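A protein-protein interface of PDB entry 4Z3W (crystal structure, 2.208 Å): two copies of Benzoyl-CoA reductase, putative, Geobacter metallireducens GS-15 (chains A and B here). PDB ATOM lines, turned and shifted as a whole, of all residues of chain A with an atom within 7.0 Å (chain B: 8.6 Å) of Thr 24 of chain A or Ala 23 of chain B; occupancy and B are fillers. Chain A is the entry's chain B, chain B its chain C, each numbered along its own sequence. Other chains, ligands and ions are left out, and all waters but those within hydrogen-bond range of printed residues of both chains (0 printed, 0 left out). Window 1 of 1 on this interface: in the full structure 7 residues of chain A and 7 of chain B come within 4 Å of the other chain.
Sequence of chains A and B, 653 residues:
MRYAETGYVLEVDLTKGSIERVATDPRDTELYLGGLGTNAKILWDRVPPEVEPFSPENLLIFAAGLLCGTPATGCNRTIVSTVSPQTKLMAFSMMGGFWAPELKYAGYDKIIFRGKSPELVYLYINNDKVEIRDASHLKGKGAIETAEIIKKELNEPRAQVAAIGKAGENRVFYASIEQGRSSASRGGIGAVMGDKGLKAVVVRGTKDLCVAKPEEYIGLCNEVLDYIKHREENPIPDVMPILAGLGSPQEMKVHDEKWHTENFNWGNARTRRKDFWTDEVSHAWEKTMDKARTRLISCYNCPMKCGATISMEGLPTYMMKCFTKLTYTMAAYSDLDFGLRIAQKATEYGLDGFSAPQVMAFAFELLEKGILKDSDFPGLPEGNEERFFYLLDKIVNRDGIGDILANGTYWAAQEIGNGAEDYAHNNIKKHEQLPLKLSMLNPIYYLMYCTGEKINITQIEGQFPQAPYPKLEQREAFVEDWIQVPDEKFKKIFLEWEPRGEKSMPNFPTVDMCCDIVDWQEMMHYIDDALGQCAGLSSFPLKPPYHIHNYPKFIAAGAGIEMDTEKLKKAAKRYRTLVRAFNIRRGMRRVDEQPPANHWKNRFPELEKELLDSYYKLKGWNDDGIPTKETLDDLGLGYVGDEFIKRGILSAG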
ATOM      1  N   ARG A   2       6.260  38.129 -18.154  1.00  0.00           N
ATOM      2  CA  ARG A   2       7.598  38.713 -18.021  1.00  0.00           C
ATOM      3  C   ARG A   2       7.548  40.232 -18.253  1.00  0.00           C
ATOM      4  O   ARG A   2       6.689  40.718 -18.980  1.00  0.00           O
ATOM      5  CB  ARG A   2       8.584  38.076 -19.012  1.00  0.00           C
ATOM      6  CG  ARG A   2       8.470  36.574 -19.194  1.00  0.00           C
ATOM      7  CD  ARG A   2       9.184  35.825 -18.092  1.00  0.00           C
ATOM      8  NE  ARG A   2      10.647  35.936 -18.158  1.00  0.00           N
ATOM      9  CZ  ARG A   2      11.444  35.101 -18.831  1.00  0.00           C
ATOM     10  NH1 ARG A   2      10.928  34.100 -19.529  1.00  0.00           N
ATOM     11  NH2 ARG A   2      12.760  35.263 -18.809  1.00  0.00           N
ATOM     12  N   GLU A   5      12.300  42.570 -20.024  1.00  0.00           N
ATOM     13  CA  GLU A   5      12.732  41.604 -21.019  1.00  0.00           C
ATOM     14  C   GLU A   5      11.482  41.098 -21.731  1.00  0.00           C
ATOM     15  O   GLU A   5      10.386  41.177 -21.177  1.00  0.00           O
ATOM     16  CB  GLU A   5      13.486  40.437 -20.362  1.00  0.00           C
ATOM     17  CG  GLU A   5      12.626  39.699 -19.325  1.00  0.00           C
ATOM     18  CD  GLU A   5      13.285  38.454 -18.757  1.00  0.00           C
ATOM     19  OE1 GLU A   5      14.352  38.057 -19.268  1.00  0.00           O
ATOM     20  OE2 GLU A   5      12.726  37.866 -17.802  1.00  0.00           O
ATOM     21  N   THR A   6      11.629  40.550 -22.933  1.00  0.00           N
ATOM     22  CA  THR A   6      10.474  39.953 -23.611  1.00  0.00           C
ATOM     23  C   THR A   6      10.307  38.454 -23.307  1.00  0.00           C
ATOM     24  O   THR A   6       9.215  37.903 -23.445  1.00  0.00           O
ATOM     25  CB  THR A   6      10.550  40.126 -25.140  1.00  0.00           C
ATOM     26  OG1 THR A   6      11.531  39.236 -25.683  1.00  0.00           O
ATOM     27  CG2 THR A   6      10.870  41.594 -25.527  1.00  0.00           C
ATOM     28  N   GLY A   7      11.386  37.788 -22.912  1.00  0.00           N
ATOM     29  CA  GLY A   7      11.311  36.374 -22.579  1.00  0.00           C
ATOM     30  C   GLY A   7      11.397  35.452 -23.783  1.00  0.00           C
ATOM     31  O   GLY A   7      11.011  34.280 -23.715  1.00  0.00           O
ATOM     32  N   TYR A   8      11.910  35.984 -24.888  1.00  0.00           N
ATOM     33  CA  TYR A   8      12.083  35.210 -26.116  1.00  0.00           C
ATOM     34  C   TYR A   8      13.394  35.529 -26.803  1.00  0.00           C
ATOM     35  O   TYR A   8      13.844  36.664 -26.784  1.00  0.00           O
ATOM     36  CB  TYR A   8      10.936  35.479 -27.089  1.00  0.00           C
ATOM     37  CG  TYR A   8       9.606  34.962 -26.606  1.00  0.00           C
ATOM     38  CD1 TYR A   8       9.341  33.592 -26.576  1.00  0.00           C
ATOM     39  CD2 TYR A   8       8.622  35.833 -26.164  1.00  0.00           C
ATOM     40  CE1 TYR A   8       8.132  33.108 -26.139  1.00  0.00           C
ATOM     41  CE2 TYR A   8       7.406  35.358 -25.718  1.00  0.00           C
ATOM     42  CZ  TYR A   8       7.169  33.991 -25.706  1.00  0.00           C
ATOM     43  OH  TYR A   8       5.964  33.495 -25.274  1.00  0.00           O
ATOM     44  N   VAL A   9      14.001  34.524 -27.412  1.00  0.00           N
ATOM     45  CA  VAL A   9      15.141  34.747 -28.276  1.00  0.00           C
ATOM     46  C   VAL A   9      14.925  34.032 -29.601  1.00  0.00           C
ATOM     47  O   VAL A   9      14.110  33.110 -29.686  1.00  0.00           O
ATOM     48  CB  VAL A   9      16.441  34.261 -27.648  1.00  0.00           C
ATOM     49  CG1 VAL A   9      16.641  34.913 -26.303  1.00  0.00           C
ATOM     50  CG2 VAL A   9      16.435  32.750 -27.536  1.00  0.00           C
ATOM     51  N   VAL A  22      12.409  30.874 -29.126  1.00  0.00           N
ATOM     52  CA  VAL A  22      12.513  30.057 -27.926  1.00  0.00           C
ATOM     53  C   VAL A  22      12.307  30.892 -26.666  1.00  0.00           C
ATOM     54  O   VAL A  22      12.957  31.919 -26.482  1.00  0.00           O
ATOM     55  CB  VAL A  22      13.876  29.362 -27.838  1.00  0.00           C
ATOM     56  CG1 VAL A  22      13.941  28.503 -26.585  1.00  0.00           C
ATOM     57  CG2 VAL A  22      14.128  28.546 -29.079  1.00  0.00           C
ATOM     58  N   ALA A  23      11.411  30.437 -25.795  1.00  0.00           N
ATOM     59  CA  ALA A  23      11.185  31.094 -24.514  1.00  0.00           C
ATOM     60  C   ALA A  23      12.432  30.960 -23.652  1.00  0.00           C
ATOM     61  O   ALA A  23      13.099  29.941 -23.699  1.00  0.00           O
ATOM     62  CB  ALA A  23       9.966  30.497 -23.815  1.00  0.00           C
ATOM     63  N   THR A  24      12.762  31.997 -22.889  1.00  0.00           N
ATOM     64  CA  THR A  24      13.932  31.947 -22.016  1.00  0.00           C
ATOM     65  C   THR A  24      13.570  31.488 -20.601  1.00  0.00           C
ATOM     66  O   THR A  24      12.404  31.469 -20.215  1.00  0.00           O
ATOM     67  CB  THR A  24      14.631  33.320 -21.909  1.00  0.00           C
ATOM     68  OG1 THR A  24      13.699  34.281 -21.413  1.00  0.00           O
ATOM     69  CG2 THR A  24      15.178  33.776 -23.256  1.00  0.00           C
ATOM     70  N   ASP A  25      14.588  31.138 -19.828  1.00  0.00           N
ATOM     71  CA  ASP A  25      14.382  30.717 -18.454  1.00  0.00           C
ATOM     72  C   ASP A  25      14.477  31.917 -17.531  1.00  0.00           C
ATOM     73  O   ASP A  25      15.535  32.527 -17.421  1.00  0.00           O
ATOM     74  CB  ASP A  25      15.406  29.637 -18.064  1.00  0.00           C
ATOM     75  CG  ASP A  25      15.276  29.184 -16.617  1.00  0.00           C
ATOM     76  OD1 ASP A  25      14.340  29.628 -15.918  1.00  0.00           O
ATOM     77  OD2 ASP A  25      16.120  28.375 -16.186  1.00  0.00           O
ATOM     78  N   PRO A  26      13.369  32.237 -16.843  1.00  0.00           N
ATOM     79  CA  PRO A  26      13.290  33.418 -15.972  1.00  0.00           C
ATOM     80  C   PRO A  26      14.327  33.375 -14.852  1.00  0.00           C
ATOM     81  O   PRO A  26      14.704  34.427 -14.330  1.00  0.00           O
ATOM     82  CB  PRO A  26      11.860  33.359 -15.421  1.00  0.00           C
ATOM     83  CG  PRO A  26      11.418  31.926 -15.621  1.00  0.00           C
ATOM     84  CD  PRO A  26      12.115  31.466 -16.860  1.00  0.00           C
ATOM     85  N   ARG A  27      14.790  32.177 -14.507  1.00  0.00           N
ATOM     86  CA  ARG A  27      15.860  32.009 -13.526  1.00  0.00           C
ATOM     87  C   ARG A  27      17.186  32.604 -13.998  1.00  0.00           C
ATOM     88  O   ARG A  27      17.952  33.133 -13.199  1.00  0.00           O
ATOM     89  CB  ARG A  27      16.065  30.535 -13.203  1.00  0.00           C
ATOM     90  CG  ARG A  27      15.707  30.160 -11.780  1.00  0.00           C
ATOM     91  CD  ARG A  27      16.758  30.619 -10.771  1.00  0.00           C
ATOM     92  NE  ARG A  27      17.320  29.517  -9.976  1.00  0.00           N
ATOM     93  CZ  ARG A  27      16.651  28.446  -9.524  1.00  0.00           C
ATOM     94  NH1 ARG A  27      15.350  28.290  -9.760  1.00  0.00           N
ATOM     95  NH2 ARG A  27      17.291  27.519  -8.814  1.00  0.00           N
ATOM     96  N   ASP A  28      17.471  32.493 -15.287  1.00  0.00           N
ATOM     97  CA  ASP A  28      18.688  33.082 -15.822  1.00  0.00           C
ATOM     98  C   ASP A  28      18.639  34.606 -15.708  1.00  0.00           C
ATOM     99  O   ASP A  28      19.672  35.264 -15.652  1.00  0.00           O
ATOM    100  CB  ASP A  28      18.898  32.661 -17.277  1.00  0.00           C
ATOM    101  CG  ASP A  28      19.318  31.208 -17.405  1.00  0.00           C
ATOM    102  OD1 ASP A  28      19.933  30.679 -16.453  1.00  0.00           O
ATOM    103  OD2 ASP A  28      19.039  30.590 -18.455  1.00  0.00           O
ATOM    104  N   THR A  29      17.440  35.172 -15.656  1.00  0.00           N
ATOM    105  CA  THR A  29      17.325  36.617 -15.481  1.00  0.00           C
ATOM    106  C   THR A  29      17.698  37.002 -14.052  1.00  0.00           C
ATOM    107  O   THR A  29      18.436  37.964 -13.830  1.00  0.00           O
ATOM    108  CB  THR A  29      15.904  37.130 -15.807  1.00  0.00           C
ATOM    109  OG1 THR A  29      15.613  36.888 -17.191  1.00  0.00           O
ATOM    110  CG2 THR A  29      15.799  38.621 -15.526  1.00  0.00           C
ATOM    111  N   ASP A 109      14.772  39.321 -27.041  1.00  0.00           N
ATOM    112  CA  ASP A 109      15.877  39.767 -26.202  1.00  0.00           C
ATOM    113  C   ASP A 109      17.239  39.514 -26.855  1.00  0.00           C
ATOM    114  O   ASP A 109      18.188  40.250 -26.608  1.00  0.00           O
ATOM    115  CB  ASP A 109      15.821  39.070 -24.844  1.00  0.00           C
ATOM    116  CG  ASP A 109      14.652  39.531 -23.998  1.00  0.00           C
ATOM    117  OD1 ASP A 109      14.436  40.771 -23.907  1.00  0.00           O
ATOM    118  OD2 ASP A 109      13.954  38.651 -23.438  1.00  0.00           O
ATOM    119  N   LYS A 110      17.335  38.460 -27.666  1.00  0.00           N
ATOM    120  CA  LYS A 110      18.590  38.085 -28.318  1.00  0.00           C
ATOM    121  C   LYS A 110      18.338  37.419 -29.662  1.00  0.00           C
ATOM    122  O   LYS A 110      17.271  36.864 -29.902  1.00  0.00           O
ATOM    123  CB  LYS A 110      19.417  37.118 -27.457  1.00  0.00           C
ATOM    124  CG  LYS A 110      19.663  37.513 -26.008  1.00  0.00           C
ATOM    125  CD  LYS A 110      20.598  36.501 -25.352  1.00  0.00           C
ATOM    126  CE  LYS A 110      20.794  36.776 -23.869  1.00  0.00           C
ATOM    127  NZ  LYS A 110      21.622  37.988 -23.608  1.00  0.00           N
ATOM    128  N   ARG B   2       5.167  32.512 -13.297  1.00  0.00           N
ATOM    129  CA  ARG B   2       4.219  31.456 -13.616  1.00  0.00           C
ATOM    130  C   ARG B   2       3.459  30.974 -12.366  1.00  0.00           C
ATOM    131  O   ARG B   2       4.010  30.952 -11.264  1.00  0.00           O
ATOM    132  CB  ARG B   2       4.963  30.288 -14.277  1.00  0.00           C
ATOM    133  CG  ARG B   2       5.989  30.717 -15.353  1.00  0.00           C
ATOM    134  CD  ARG B   2       5.284  31.166 -16.610  1.00  0.00           C
ATOM    135  NE  ARG B   2       4.662  30.053 -17.330  1.00  0.00           N
ATOM    136  CZ  ARG B   2       5.316  29.194 -18.117  1.00  0.00           C
ATOM    137  NH1 ARG B   2       6.631  29.294 -18.292  1.00  0.00           N
ATOM    138  NH2 ARG B   2       4.653  28.234 -18.752  1.00  0.00           N
ATOM    139  N   THR B   6       4.600  24.914 -12.859  1.00  0.00           N
ATOM    140  CA  THR B   6       5.911  25.283 -12.349  1.00  0.00           C
ATOM    141  C   THR B   6       6.707  26.052 -13.384  1.00  0.00           C
ATOM    142  O   THR B   6       7.578  26.843 -13.034  1.00  0.00           O
ATOM    143  CB  THR B   6       6.717  24.058 -11.951  1.00  0.00           C
ATOM    144  OG1 THR B   6       7.092  23.354 -13.137  1.00  0.00           O
ATOM    145  CG2 THR B   6       5.882  23.135 -11.057  1.00  0.00           C
ATOM    146  N   GLY B   7       6.431  25.784 -14.657  1.00  0.00           N
ATOM    147  CA  GLY B   7       7.118  26.450 -15.751  1.00  0.00           C
ATOM    148  C   GLY B   7       8.338  25.717 -16.297  1.00  0.00           C
ATOM    149  O   GLY B   7       9.010  26.223 -17.195  1.00  0.00           O
ATOM    150  N   TYR B   8       8.636  24.534 -15.756  1.00  0.00           N
ATOM    151  CA  TYR B   8       9.789  23.744 -16.208  1.00  0.00           C
ATOM    152  C   TYR B   8       9.463  22.290 -16.528  1.00  0.00           C
ATOM    153  O   TYR B   8       8.568  21.697 -15.927  1.00  0.00           O
ATOM    154  CB  TYR B   8      10.887  23.732 -15.153  1.00  0.00           C
ATOM    155  CG  TYR B   8      11.449  25.072 -14.822  1.00  0.00           C
ATOM    156  CD1 TYR B   8      12.400  25.666 -15.643  1.00  0.00           C
ATOM    157  CD2 TYR B   8      11.049  25.738 -13.677  1.00  0.00           C
ATOM    158  CE1 TYR B   8      12.929  26.897 -15.338  1.00  0.00           C
ATOM    159  CE2 TYR B   8      11.575  26.957 -13.356  1.00  0.00           C
ATOM    160  CZ  TYR B   8      12.510  27.546 -14.197  1.00  0.00           C
ATOM    161  OH  TYR B   8      13.034  28.774 -13.876  1.00  0.00           O
ATOM    162  N   VAL B   9      10.234  21.714 -17.446  1.00  0.00           N
ATOM    163  CA  VAL B   9      10.203  20.281 -17.691  1.00  0.00           C
ATOM    164  C   VAL B   9      11.608  19.710 -17.596  1.00  0.00           C
ATOM    165  O   VAL B   9      12.586  20.441 -17.731  1.00  0.00           O
ATOM    166  CB  VAL B   9       9.619  19.949 -19.068  1.00  0.00           C
ATOM    167  CG1 VAL B   9       8.237  20.527 -19.195  1.00  0.00           C
ATOM    168  CG2 VAL B   9      10.526  20.491 -20.171  1.00  0.00           C
ATOM    169  N   LEU B  10      11.706  18.408 -17.350  1.00  0.00           N
ATOM    170  CA  LEU B  10      12.986  17.710 -17.452  1.00  0.00           C
ATOM    171  C   LEU B  10      13.084  16.994 -18.787  1.00  0.00           C
ATOM    172  O   LEU B  10      12.202  16.202 -19.147  1.00  0.00           O
ATOM    173  CB  LEU B  10      13.174  16.695 -16.316  1.00  0.00           C
ATOM    174  CG  LEU B  10      13.418  17.256 -14.915  1.00  0.00           C
ATOM    175  CD1 LEU B  10      13.299  16.148 -13.907  1.00  0.00           C
ATOM    176  CD2 LEU B  10      14.780  17.931 -14.820  1.00  0.00           C
ATOM    177  N   GLU B  11      14.159  17.280 -19.515  1.00  0.00           N
ATOM    178  CA  GLU B  11      14.497  16.549 -20.729  1.00  0.00           C
ATOM    179  C   GLU B  11      15.513  15.475 -20.399  1.00  0.00           C
ATOM    180  O   GLU B  11      16.613  15.783 -19.928  1.00  0.00           O
ATOM    181  CB  GLU B  11      15.059  17.492 -21.807  1.00  0.00           C
ATOM    182  CG  GLU B  11      14.031  18.426 -22.395  1.00  0.00           C
ATOM    183  CD  GLU B  11      12.992  17.688 -23.216  1.00  0.00           C
ATOM    184  OE1 GLU B  11      13.156  16.460 -23.408  1.00  0.00           O
ATOM    185  OE2 GLU B  11      12.018  18.331 -23.668  1.00  0.00           O
ATOM    186  N   GLU B  20      18.384  17.401 -18.355  1.00  0.00           N
ATOM    187  CA  GLU B  20      18.361  18.855 -18.526  1.00  0.00           C
ATOM    188  C   GLU B  20      17.027  19.475 -18.144  1.00  0.00           C
ATOM    189  O   GLU B  20      15.974  18.996 -18.563  1.00  0.00           O
ATOM    190  CB  GLU B  20      18.692  19.197 -19.964  1.00  0.00           C
ATOM    191  CG  GLU B  20      18.812  20.666 -20.249  1.00  0.00           C
ATOM    192  CD  GLU B  20      19.290  20.901 -21.659  1.00  0.00           C
ATOM    193  OE1 GLU B  20      20.076  20.060 -22.152  1.00  0.00           O
ATOM    194  OE2 GLU B  20      18.869  21.902 -22.276  1.00  0.00           O
ATOM    195  N   ARG B  21      17.066  20.531 -17.337  1.00  0.00           N
ATOM    196  CA  ARG B  21      15.843  21.265 -17.020  1.00  0.00           C
ATOM    197  C   ARG B  21      15.615  22.377 -18.038  1.00  0.00           C
ATOM    198  O   ARG B  21      16.480  23.220 -18.220  1.00  0.00           O
ATOM    199  CB  ARG B  21      15.892  21.869 -15.618  1.00  0.00           C
ATOM    200  CG  ARG B  21      14.601  22.594 -15.268  1.00  0.00           C
ATOM    201  CD  ARG B  21      14.588  23.165 -13.855  1.00  0.00           C
ATOM    202  NE  ARG B  21      15.277  24.447 -13.780  1.00  0.00           N
ATOM    203  CZ  ARG B  21      15.154  25.306 -12.773  1.00  0.00           C
ATOM    204  NH1 ARG B  21      14.362  25.029 -11.748  1.00  0.00           N
ATOM    205  NH2 ARG B  21      15.823  26.450 -12.792  1.00  0.00           N
ATOM    206  N   VAL B  22      14.444  22.383 -18.673  1.00  0.00           N
ATOM    207  CA  VAL B  22      14.111  23.392 -19.670  1.00  0.00           C
ATOM    208  C   VAL B  22      12.854  24.184 -19.303  1.00  0.00           C
ATOM    209  O   VAL B  22      11.848  23.607 -18.891  1.00  0.00           O
ATOM    210  CB  VAL B  22      13.899  22.762 -21.064  1.00  0.00           C
ATOM    211  CG1 VAL B  22      13.697  23.873 -22.117  1.00  0.00           C
ATOM    212  CG2 VAL B  22      15.080  21.883 -21.438  1.00  0.00           C
ATOM    213  N   ALA B  23      12.906  25.507 -19.473  1.00  0.00           N
ATOM    214  CA  ALA B  23      11.752  26.351 -19.183  1.00  0.00           C
ATOM    215  C   ALA B  23      10.753  26.256 -20.316  1.00  0.00           C
ATOM    216  O   ALA B  23      11.130  26.137 -21.472  1.00  0.00           O
ATOM    217  CB  ALA B  23      12.172  27.800 -18.971  1.00  0.00           C
ATOM    218  N   THR B  24       9.472  26.304 -19.988  1.00  0.00           N
ATOM    219  CA  THR B  24       8.469  26.194 -21.026  1.00  0.00           C
ATOM    220  C   THR B  24       8.042  27.557 -21.558  1.00  0.00           C
ATOM    221  O   THR B  24       8.420  28.619 -21.049  1.00  0.00           O
ATOM    222  CB  THR B  24       7.207  25.437 -20.541  1.00  0.00           C
ATOM    223  OG1 THR B  24       6.771  25.976 -19.292  1.00  0.00           O
ATOM    224  CG2 THR B  24       7.502  23.960 -20.369  1.00  0.00           C
ATOM    225  N   ASP B  25       7.221  27.476 -22.589  1.00  0.00           N
ATOM    226  CA  ASP B  25       6.715  28.612 -23.303  1.00  0.00           C
ATOM    227  C   ASP B  25       5.286  28.884 -22.869  1.00  0.00           C
ATOM    228  O   ASP B  25       4.378  28.141 -23.234  1.00  0.00           O
ATOM    229  CB  ASP B  25       6.796  28.332 -24.808  1.00  0.00           C
ATOM    230  CG  ASP B  25       6.311  29.489 -25.652  1.00  0.00           C
ATOM    231  OD1 ASP B  25       5.768  30.472 -25.102  1.00  0.00           O
ATOM    232  OD2 ASP B  25       6.463  29.392 -26.884  1.00  0.00           O
ATOM    233  N   PRO B  26       5.079  29.985 -22.126  1.00  0.00           N
ATOM    234  CA  PRO B  26       3.779  30.365 -21.560  1.00  0.00           C
ATOM    235  C   PRO B  26       2.689  30.538 -22.616  1.00  0.00           C
ATOM    236  O   PRO B  26       1.507  30.594 -22.279  1.00  0.00           O
ATOM    237  CB  PRO B  26       4.080  31.703 -20.869  1.00  0.00           C
ATOM    238  CG  PRO B  26       5.284  32.228 -21.581  1.00  0.00           C
ATOM    239  CD  PRO B  26       6.104  31.014 -21.883  1.00  0.00           C
ATOM    240  N   ASP B  28       2.233  28.239 -24.935  1.00  0.00           N
ATOM    241  CA  ASP B  28       1.705  26.877 -24.995  1.00  0.00           C
ATOM    242  C   ASP B  28       0.681  26.614 -23.883  1.00  0.00           C
ATOM    243  O   ASP B  28      -0.254  25.830 -24.059  1.00  0.00           O
ATOM    244  CB  ASP B  28       2.837  25.855 -24.911  1.00  0.00           C
ATOM    245  CG  ASP B  28       3.630  25.755 -26.204  1.00  0.00           C
ATOM    246  OD1 ASP B  28       3.075  26.104 -27.268  1.00  0.00           O
ATOM    247  OD2 ASP B  28       4.801  25.323 -26.150  1.00  0.00           O
ATOM    248  N   ASP B 109       6.752  20.319 -14.389  1.00  0.00           N
ATOM    249  CA  ASP B 109       5.456  20.072 -15.007  1.00  0.00           C
ATOM    250  C   ASP B 109       5.443  18.733 -15.748  1.00  0.00           C
ATOM    251  O   ASP B 109       4.423  18.054 -15.792  1.00  0.00           O
ATOM    252  CB  ASP B 109       5.097  21.207 -15.973  1.00  0.00           C
ATOM    253  CG  ASP B 109       4.803  22.516 -15.255  1.00  0.00           C
ATOM    254  OD1 ASP B 109       4.196  22.456 -14.158  1.00  0.00           O
ATOM    255  OD2 ASP B 109       5.181  23.594 -15.786  1.00  0.00           O
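Of the 16 printed residues of chain A, 6 touch a printed residue of chain B. Hydrophobic or aromatic side chains of chain A within 4 Å of the printed part of chain B: Tyr 8, Ala 23 and Pro 26. Of the 16 printed residues of chain B, 6 touch a printed residue of chain A. Among the printed residues, Asp or Glu carboxylates within 4 Å of a Lys or Arg side-chain nitrogen of the other chain: Asp 25 of chain A with Arg 21 of chain B.
OH of Tyr 8 of chain A lies within hydrogen-bond range of OD1 of Asp 25 of chain B (3.0 Å). OH of Tyr 8 of chain B is in hydrogen-bond range of OD1 of Asp 25 of chain A (2.6 Å). The side-chain carboxylate (OD2) of Asp 25 of chain A is in salt-bridge range of the guanidinium group (NH2) of Arg 21 of chain B (3.9 Å).
Tyr 8 of chain A touches Asp 25 of chain B, and with the chains exchanged Asp 25 of chain A touches Tyr 8 of chain B. Tyr 8 of chain A touches Pro 26 of chain B, and with the chains exchanged Pro 26 of chain A touches Tyr 8 of chain B. Ala 23 of chain A touches Thr 24 of chain B, and with the chains exchanged Thr 24 of chain A touches Ala 23 of chain B. Ala 23 of chain A touches Asp 25 of chain B, and with the chains exchanged Asp 25 of chain A touches Ala 23 of chain B. Positions printed for both chains: 2, 6, 7, 8, 9, 22, 23, 24, 25, 26, 28 and 109.
NH2 of Arg 2 of chain A sits at hydrogen-bond distance from OG1 of Thr 24 of chain A, at 2.9 Å. O of Gly 7 of chain A lies within hydrogen-bond range of N of Thr 24 of chain A, 3.0 Å away. The backbone NH of Asp 109 of chain A lies within hydrogen-bond range of the backbone carbonyl oxygen of Tyr 8 of chain A (2.8 Å). The backbone NH (N) of Arg 27 of chain A sits at hydrogen-bond distance from the side-chain carboxylate (OD1) of Asp 25 of chain A. NH2 of Arg 2 of chain B lies within hydrogen-bond range of OG1 of Thr 24 of chain B (3.1 Å). The side-chain hydroxyl of Thr 6 of chain B sits at hydrogen-bond distance from the backbone NH of Tyr 8 of chain B.
No residue of chain B comes within 4 Å of Gly 7 of chain A. Ala 23 of chain A touches just these residues of chain B: Thr 24 (3.7 Å) and Asp 25 (3.8 Å). Thr 24 of chain A touches one residue of chain B. Of the printed residues of chain B, Asp 25 of chain A touches Tyr 8, Arg 21 and Ala 23. Printed residues of chain B within 4 Å of Arg 27 of chain A: Tyr 8 and Arg 21. Gly 7 of chain B touches none of the printed residues of chain A. Ala 23 of chain B touches just these residues of chain A: Thr 24 and Asp 25. The nearest printed residue of chain B that does not touch Tyr 8 of chain A is Asp 28 of chain B (6.5 Å).
Among the printed residues, merely in contact across the chains: Arg 27 of chain A with Tyr 8 of chain B (3.6 Å), Arg 27 of chain A with Arg 21 of chain B (3.6 Å), Ala 23 of chain A with Thr 24 of chain B (3.7 Å), Asp 25 of chain A with Ala 23 of chain B (3.7 Å), Ala 23 of chain A with Asp 25 of chain B (3.8 Å), Thr 24 of chain A with Ala 23 of chain B (3.9 Å), Pro 26 of chain A with Tyr 8 of chain B (3.9 Å) and Tyr 8 of chain A with Pro 26 of chain B (3.96 Å).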
